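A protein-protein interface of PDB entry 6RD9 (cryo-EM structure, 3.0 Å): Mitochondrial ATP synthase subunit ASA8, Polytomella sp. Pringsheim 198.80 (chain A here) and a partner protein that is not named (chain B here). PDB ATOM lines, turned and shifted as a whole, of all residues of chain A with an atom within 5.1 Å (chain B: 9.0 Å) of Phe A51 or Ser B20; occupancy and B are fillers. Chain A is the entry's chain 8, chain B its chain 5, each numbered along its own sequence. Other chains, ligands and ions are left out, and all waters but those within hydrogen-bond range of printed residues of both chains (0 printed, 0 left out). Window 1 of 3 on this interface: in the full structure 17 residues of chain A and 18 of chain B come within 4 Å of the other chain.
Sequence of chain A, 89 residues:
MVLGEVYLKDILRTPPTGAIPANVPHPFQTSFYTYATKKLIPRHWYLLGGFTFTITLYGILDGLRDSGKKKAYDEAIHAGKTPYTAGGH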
ATOM      1  N   LEU A  47       5.076  11.026  21.480  1.00  0.00           N
ATOM      2  CA  LEU A  47       6.181  10.177  21.050  1.00  0.00           C
ATOM      3  C   LEU A  47       6.625   9.240  22.144  1.00  0.00           C
ATOM      4  O   LEU A  47       6.940   8.083  21.875  1.00  0.00           O
ATOM      5  CB  LEU A  47       7.390  10.981  20.626  1.00  0.00           C
ATOM      6  CG  LEU A  47       7.646  11.289  19.183  1.00  0.00           C
ATOM      7  CD1 LEU A  47       9.051  11.742  19.111  1.00  0.00           C
ATOM      8  CD2 LEU A  47       7.471  10.055  18.374  1.00  0.00           C
ATOM      9  N   LEU A  48       6.715   9.730  23.370  1.00  0.00           N
ATOM     10  CA  LEU A  48       7.149   8.880  24.461  1.00  0.00           C
ATOM     11  C   LEU A  48       6.110   7.831  24.785  1.00  0.00           C
ATOM     12  O   LEU A  48       6.449   6.767  25.292  1.00  0.00           O
ATOM     13  CB  LEU A  48       7.435   9.713  25.693  1.00  0.00           C
ATOM     14  CG  LEU A  48       8.432  10.847  25.587  1.00  0.00           C
ATOM     15  CD1 LEU A  48       8.663  11.342  26.977  1.00  0.00           C
ATOM     16  CD2 LEU A  48       9.707  10.393  24.951  1.00  0.00           C
ATOM     17  N   GLY A  49       4.843   8.116  24.518  1.00  0.00           N
ATOM     18  CA  GLY A  49       3.839   7.083  24.600  1.00  0.00           C
ATOM     19  C   GLY A  49       3.924   6.107  23.460  1.00  0.00           C
ATOM     20  O   GLY A  49       3.598   4.936  23.629  1.00  0.00           O
ATOM     21  N   GLY A  50       4.348   6.559  22.289  1.00  0.00           N
ATOM     22  CA  GLY A  50       4.489   5.657  21.168  1.00  0.00           C
ATOM     23  C   GLY A  50       5.721   4.790  21.253  1.00  0.00           C
ATOM     24  O   GLY A  50       5.723   3.672  20.749  1.00  0.00           O
ATOM     25  N   PHE A  51       6.794   5.297  21.852  1.00  0.00           N
ATOM     26  CA  PHE A  51       7.947   4.454  22.122  1.00  0.00           C
ATOM     27  C   PHE A  51       7.664   3.487  23.253  1.00  0.00           C
ATOM     28  O   PHE A  51       8.249   2.412  23.299  1.00  0.00           O
ATOM     29  CB  PHE A  51       9.163   5.303  22.477  1.00  0.00           C
ATOM     30  CG  PHE A  51       9.755   6.040  21.325  1.00  0.00           C
ATOM     31  CD1 PHE A  51       9.911   5.430  20.111  1.00  0.00           C
ATOM     32  CD2 PHE A  51      10.186   7.334  21.471  1.00  0.00           C
ATOM     33  CE1 PHE A  51      10.449   6.095  19.050  1.00  0.00           C
ATOM     34  CE2 PHE A  51      10.736   8.000  20.417  1.00  0.00           C
ATOM     35  CZ  PHE A  51      10.858   7.377  19.205  1.00  0.00           C
ATOM     36  N   THR A  52       6.788   3.857  24.181  1.00  0.00           N
ATOM     37  CA  THR A  52       6.424   2.961  25.271  1.00  0.00           C
ATOM     38  C   THR A  52       5.522   1.847  24.778  1.00  0.00           C
ATOM     39  O   THR A  52       5.626   0.710  25.242  1.00  0.00           O
ATOM     40  CB  THR A  52       5.746   3.753  26.381  1.00  0.00           C
ATOM     41  OG1 THR A  52       6.649   4.752  26.845  1.00  0.00           O
ATOM     42  CG2 THR A  52       5.389   2.896  27.551  1.00  0.00           C
ATOM     43  N   PHE A  53       4.645   2.146  23.826  1.00  0.00           N
ATOM     44  CA  PHE A  53       3.780   1.119  23.269  1.00  0.00           C
ATOM     45  C   PHE A  53       4.572   0.069  22.513  1.00  0.00           C
ATOM     46  O   PHE A  53       4.252  -1.114  22.581  1.00  0.00           O
ATOM     47  CB  PHE A  53       2.748   1.746  22.351  1.00  0.00           C
ATOM     48  CG  PHE A  53       1.873   0.752  21.675  1.00  0.00           C
ATOM     49  CD1 PHE A  53       0.866   0.133  22.366  1.00  0.00           C
ATOM     50  CD2 PHE A  53       2.049   0.442  20.345  1.00  0.00           C
ATOM     51  CE1 PHE A  53       0.064  -0.772  21.752  1.00  0.00           C
ATOM     52  CE2 PHE A  53       1.252  -0.469  19.736  1.00  0.00           C
ATOM     53  CZ  PHE A  53       0.259  -1.072  20.438  1.00  0.00           C
ATOM     54  N   THR A  54       5.609   0.473  21.800  1.00  0.00           N
ATOM     55  CA  THR A  54       6.375  -0.477  21.012  1.00  0.00           C
ATOM     56  C   THR A  54       7.237  -1.369  21.881  1.00  0.00           C
ATOM     57  O   THR A  54       7.341  -2.562  21.614  1.00  0.00           O
ATOM     58  CB  THR A  54       7.230   0.279  20.023  1.00  0.00           C
ATOM     59  OG1 THR A  54       6.378   1.093  19.231  1.00  0.00           O
ATOM     60  CG2 THR A  54       7.943  -0.640  19.119  1.00  0.00           C
ATOM     61  N   ILE A  55       7.835  -0.826  22.934  1.00  0.00           N
ATOM     62  CA  ILE A  55       8.663  -1.631  23.819  1.00  0.00           C
ATOM     63  C   ILE A  55       7.801  -2.604  24.608  1.00  0.00           C
ATOM     64  O   ILE A  55       8.201  -3.738  24.877  1.00  0.00           O
ATOM     65  CB  ILE A  55       9.486  -0.698  24.719  1.00  0.00           C
ATOM     66  CG1 ILE A  55      10.463   0.083  23.876  1.00  0.00           C
ATOM     67  CG2 ILE A  55      10.253  -1.442  25.753  1.00  0.00           C
ATOM     68  CD1 ILE A  55      11.064   1.217  24.593  1.00  0.00           C
ATOM     69  N   GLN B   9      12.527  -6.804  21.904  1.00  0.00           N
ATOM     70  CA  GLN B   9      12.370  -5.673  22.799  1.00  0.00           C
ATOM     71  C   GLN B   9      13.678  -4.940  22.993  1.00  0.00           C
ATOM     72  O   GLN B   9      13.677  -3.741  23.250  1.00  0.00           O
ATOM     73  CB  GLN B   9      11.848  -6.146  24.140  1.00  0.00           C
ATOM     74  CG  GLN B   9      11.323  -5.079  25.018  1.00  0.00           C
ATOM     75  CD  GLN B   9      10.794  -5.636  26.285  1.00  0.00           C
ATOM     76  OE1 GLN B   9      11.431  -6.458  26.912  1.00  0.00           O
ATOM     77  NE2 GLN B   9       9.612  -5.212  26.669  1.00  0.00           N
ATOM     78  N   ALA B  12      13.892  -2.874  19.813  1.00  0.00           N
ATOM     79  CA  ALA B  12      12.922  -1.798  19.811  1.00  0.00           C
ATOM     80  C   ALA B  12      13.284  -0.732  20.815  1.00  0.00           C
ATOM     81  O   ALA B  12      13.013   0.441  20.579  1.00  0.00           O
ATOM     82  CB  ALA B  12      11.532  -2.329  20.117  1.00  0.00           C
ATOM     83  N   ALA B  13      13.899  -1.112  21.928  1.00  0.00           N
ATOM     84  CA  ALA B  13      14.322  -0.133  22.909  1.00  0.00           C
ATOM     85  C   ALA B  13      15.600   0.555  22.508  1.00  0.00           C
ATOM     86  O   ALA B  13      15.866   1.647  22.990  1.00  0.00           O
ATOM     87  CB  ALA B  13      14.515  -0.781  24.264  1.00  0.00           C
ATOM     88  N   THR B  14      16.425  -0.065  21.676  1.00  0.00           N
ATOM     89  CA  THR B  14      17.558   0.654  21.115  1.00  0.00           C
ATOM     90  C   THR B  14      17.084   1.718  20.144  1.00  0.00           C
ATOM     91  O   THR B  14      17.669   2.796  20.070  1.00  0.00           O
ATOM     92  CB  THR B  14      18.515  -0.319  20.446  1.00  0.00           C
ATOM     93  OG1 THR B  14      18.921  -1.302  21.395  1.00  0.00           O
ATOM     94  CG2 THR B  14      19.731   0.364  19.953  1.00  0.00           C
ATOM     95  N   ALA B  15      15.994   1.465  19.430  1.00  0.00           N
ATOM     96  CA  ALA B  15      15.438   2.476  18.544  1.00  0.00           C
ATOM     97  C   ALA B  15      14.792   3.602  19.315  1.00  0.00           C
ATOM     98  O   ALA B  15      14.810   4.741  18.864  1.00  0.00           O
ATOM     99  CB  ALA B  15      14.411   1.860  17.611  1.00  0.00           C
ATOM    100  N   ALA B  16      14.225   3.314  20.470  1.00  0.00           N
ATOM    101  CA  ALA B  16      13.590   4.355  21.254  1.00  0.00           C
ATOM    102  C   ALA B  16      14.598   5.154  22.039  1.00  0.00           C
ATOM    103  O   ALA B  16      14.329   6.291  22.391  1.00  0.00           O
ATOM    104  CB  ALA B  16      12.562   3.748  22.191  1.00  0.00           C
ATOM    105  N   VAL B  17      15.751   4.577  22.345  1.00  0.00           N
ATOM    106  CA  VAL B  17      16.801   5.325  23.014  1.00  0.00           C
ATOM    107  C   VAL B  17      17.525   6.211  22.023  1.00  0.00           C
ATOM    108  O   VAL B  17      17.839   7.360  22.322  1.00  0.00           O
ATOM    109  CB  VAL B  17      17.742   4.349  23.740  1.00  0.00           C
ATOM    110  CG1 VAL B  17      19.043   4.976  24.094  1.00  0.00           C
ATOM    111  CG2 VAL B  17      17.094   3.886  24.986  1.00  0.00           C
ATOM    112  N   VAL B  18      17.753   5.719  20.814  1.00  0.00           N
ATOM    113  CA  VAL B  18      18.416   6.527  19.801  1.00  0.00           C
ATOM    114  C   VAL B  18      17.507   7.651  19.333  1.00  0.00           C
ATOM    115  O   VAL B  18      17.927   8.800  19.241  1.00  0.00           O
ATOM    116  CB  VAL B  18      18.890   5.644  18.641  1.00  0.00           C
ATOM    117  CG1 VAL B  18      19.323   6.466  17.509  1.00  0.00           C
ATOM    118  CG2 VAL B  18      20.042   4.829  19.079  1.00  0.00           C
ATOM    119  N   ALA B  19      16.237   7.364  19.089  1.00  0.00           N
ATOM    120  CA  ALA B  19      15.361   8.413  18.593  1.00  0.00           C
ATOM    121  C   ALA B  19      14.898   9.372  19.674  1.00  0.00           C
ATOM    122  O   ALA B  19      14.423  10.452  19.343  1.00  0.00           O
ATOM    123  CB  ALA B  19      14.162   7.811  17.893  1.00  0.00           C
ATOM    124  N   SER B  20      15.005   9.023  20.947  1.00  0.00           N
ATOM    125  CA  SER B  20      14.729   9.996  21.992  1.00  0.00           C
ATOM    126  C   SER B  20      15.949  10.790  22.362  1.00  0.00           C
ATOM    127  O   SER B  20      15.822  11.860  22.945  1.00  0.00           O
ATOM    128  CB  SER B  20      14.220   9.332  23.254  1.00  0.00           C
ATOM    129  OG  SER B  20      13.068   8.590  22.969  1.00  0.00           O
ATOM    130  N   TRP B  21      17.131  10.284  22.079  1.00  0.00           N
ATOM    131  CA  TRP B  21      18.295  11.129  22.218  1.00  0.00           C
ATOM    132  C   TRP B  21      18.344  12.150  21.108  1.00  0.00           C
ATOM    133  O   TRP B  21      18.747  13.286  21.334  1.00  0.00           O
ATOM    134  CB  TRP B  21      19.560  10.303  22.220  1.00  0.00           C
ATOM    135  CG  TRP B  21      20.755  11.101  22.458  1.00  0.00           C
ATOM    136  CD1 TRP B  21      21.299  11.398  23.649  1.00  0.00           C
ATOM    137  CD2 TRP B  21      21.582  11.712  21.476  1.00  0.00           C
ATOM    138  NE1 TRP B  21      22.404  12.158  23.479  1.00  0.00           N
ATOM    139  CE2 TRP B  21      22.597  12.362  22.144  1.00  0.00           C
ATOM    140  CE3 TRP B  21      21.556  11.767  20.087  1.00  0.00           C
ATOM    141  CZ2 TRP B  21      23.569  13.054  21.491  1.00  0.00           C
ATOM    142  CZ3 TRP B  21      22.515  12.453  19.449  1.00  0.00           C
ATOM    143  CH2 TRP B  21      23.510  13.084  20.142  1.00  0.00           C
ATOM    144  N   VAL B  22      17.977  11.764  19.894  1.00  0.00           N
ATOM    145  CA  VAL B  22      17.934  12.717  18.798  1.00  0.00           C
ATOM    146  C   VAL B  22      16.827  13.728  19.028  1.00  0.00           C
ATOM    147  O   VAL B  22      16.965  14.894  18.677  1.00  0.00           O
ATOM    148  CB  VAL B  22      17.792  11.972  17.464  1.00  0.00           C
ATOM    149  CG1 VAL B  22      17.684  12.900  16.328  1.00  0.00           C
ATOM    150  CG2 VAL B  22      18.982  11.132  17.252  1.00  0.00           C
ATOM    151  N   LEU B  23      15.752  13.332  19.685  1.00  0.00           N
ATOM    152  CA  LEU B  23      14.726  14.298  20.038  1.00  0.00           C
ATOM    153  C   LEU B  23      15.212  15.256  21.097  1.00  0.00           C
ATOM    154  O   LEU B  23      14.980  16.456  20.992  1.00  0.00           O
ATOM    155  CB  LEU B  23      13.481  13.597  20.529  1.00  0.00           C
ATOM    156  CG  LEU B  23      12.347  14.519  20.881  1.00  0.00           C
ATOM    157  CD1 LEU B  23      11.863  15.121  19.637  1.00  0.00           C
ATOM    158  CD2 LEU B  23      11.301  13.701  21.496  1.00  0.00           C
ATOM    159  N   TRP B  24      15.896  14.753  22.114  1.00  0.00           N
ATOM    160  CA  TRP B  24      16.460  15.627  23.127  1.00  0.00           C
ATOM    161  C   TRP B  24      17.529  16.517  22.540  1.00  0.00           C
ATOM    162  O   TRP B  24      17.539  17.709  22.796  1.00  0.00           O
ATOM    163  CB  TRP B  24      17.032  14.818  24.283  1.00  0.00           C
ATOM    164  CG  TRP B  24      17.860  15.640  25.175  1.00  0.00           C
ATOM    165  CD1 TRP B  24      17.435  16.423  26.172  1.00  0.00           C
ATOM    166  CD2 TRP B  24      19.276  15.769  25.145  1.00  0.00           C
ATOM    167  NE1 TRP B  24      18.483  17.048  26.764  1.00  0.00           N
ATOM    168  CE2 TRP B  24      19.630  16.663  26.136  1.00  0.00           C
ATOM    169  CE3 TRP B  24      20.274  15.230  24.347  1.00  0.00           C
ATOM    170  CZ2 TRP B  24      20.929  17.015  26.363  1.00  0.00           C
ATOM    171  CZ3 TRP B  24      21.549  15.585  24.575  1.00  0.00           C
ATOM    172  CH2 TRP B  24      21.871  16.464  25.566  1.00  0.00           C
ATOM    173  N   HIS B  25      18.426  15.966  21.737  1.00  0.00           N
ATOM    174  CA  HIS B  25      19.520  16.759  21.206  1.00  0.00           C
ATOM    175  C   HIS B  25      19.050  17.814  20.241  1.00  0.00           C
ATOM    176  O   HIS B  25      19.606  18.901  20.212  1.00  0.00           O
ATOM    177  CB  HIS B  25      20.514  15.879  20.507  1.00  0.00           C
ATOM    178  CG  HIS B  25      21.832  16.529  20.334  1.00  0.00           C
ATOM    179  ND1 HIS B  25      22.226  17.109  19.158  1.00  0.00           N
ATOM    180  CD2 HIS B  25      22.831  16.742  21.212  1.00  0.00           C
ATOM    181  CE1 HIS B  25      23.427  17.626  19.310  1.00  0.00           C
ATOM    182  NE2 HIS B  25      23.813  17.421  20.550  1.00  0.00           N
ATOM    183  N   LEU B  26      18.019  17.533  19.476  1.00  0.00           N
ATOM    184  CA  LEU B  26      17.473  18.535  18.588  1.00  0.00           C
ATOM    185  C   LEU B  26      16.777  19.633  19.368  1.00  0.00           C
ATOM    186  O   LEU B  26      17.027  20.809  19.136  1.00  0.00           O
ATOM    187  CB  LEU B  26      16.514  17.871  17.635  1.00  0.00           C
ATOM    188  CG  LEU B  26      15.881  18.628  16.520  1.00  0.00           C
ATOM    189  CD1 LEU B  26      16.870  18.734  15.434  1.00  0.00           C
ATOM    190  CD2 LEU B  26      14.745  17.791  16.138  1.00  0.00           C
ATOM    191  N   ASP B  27      15.922  19.269  20.315  1.00  0.00           N
ATOM    192  CA  ASP B  27      15.123  20.249  21.036  1.00  0.00           C
ATOM    193  C   ASP B  27      15.934  21.115  21.958  1.00  0.00           C
ATOM    194  O   ASP B  27      15.534  22.236  22.256  1.00  0.00           O
ATOM    195  CB  ASP B  27      14.106  19.566  21.898  1.00  0.00           C
ATOM    196  CG  ASP B  27      12.807  19.413  21.250  1.00  0.00           C
ATOM    197  OD1 ASP B  27      12.467  20.219  20.376  1.00  0.00           O
ATOM    198  OD2 ASP B  27      12.075  18.517  21.676  1.00  0.00           O
ATOM    199  N   THR B  28      17.023  20.594  22.473  1.00  0.00           N
ATOM    200  CA  THR B  28      17.790  21.246  23.511  1.00  0.00           C
ATOM    201  C   THR B  28      19.046  21.895  22.965  1.00  0.00           C
ATOM    202  O   THR B  28      19.346  23.030  23.300  1.00  0.00           O
ATOM    203  CB  THR B  28      18.115  20.218  24.581  1.00  0.00           C
ATOM    204  OG1 THR B  28      16.949  19.951  25.343  1.00  0.00           O
ATOM    205  CG2 THR B  28      19.163  20.653  25.469  1.00  0.00           C
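The backbone carbonyl oxygen of Ile A55 lies within hydrogen-bond range of the side-chain amide nitrogen of Gln B9, 2.7 Å away.
O of Ala B16 is in hydrogen-bond range of OG of Ser B20, at 2.7 Å.
Leu B23 touches Leu A47. Ala B16 touches Phe A51 (CB to CG, 3.7 Å). Phe A51 touches Ala B19. Phe A51 touches Ser B20. Ile A55 touches Ala B13 (CD1 to CA, 3.9 Å). Ala B16 touches Ile A55 (CB to CD1, 3.8 Å).
Phe A51 touches just these residues of chain B: Ala B16, Ala B19 and Ser B20. Of chain A, only Phe A51 comes within 4 Å of Ser B20. No residue of chain B comes within 4 Å of Gly A49. Gly A50 touches none of the printed residues of chain B. No residue of chain B comes within 4 Å of Thr A52. Printed residues of chain B within 4 Å of Ile A55: Gln B9, Ala B13 and Ala B16. Printed residues of chain A within 4 Å of Leu B23: Leu A47 (3.8 Å). Printed residues of chain A within 4 Å of Ala B13: Ile A55 (3.9 Å). Of the printed residues of chain A, Ala B19 touches Phe A51. Ala B15 touches none of the printed residues of chain A. Ala B12 touches none of the printed residues of chain A. The nearest printed residue of chain A that does not touch Leu B23 is Leu A48 (5.0 Å).
Hydrophobic or aromatic side chains of chain A that line the printed part of chain B: Leu A47, Phe A51 and Ile A55. Hydrophobic or aromatic side chains of chain B that line the printed part of chain A: Ala B16, Ala B19 and Leu B23. Among the printed residues, no Asp or Glu carboxylate lies within 4 Å of a Lys or Arg side-chain nitrogen of the other chain.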
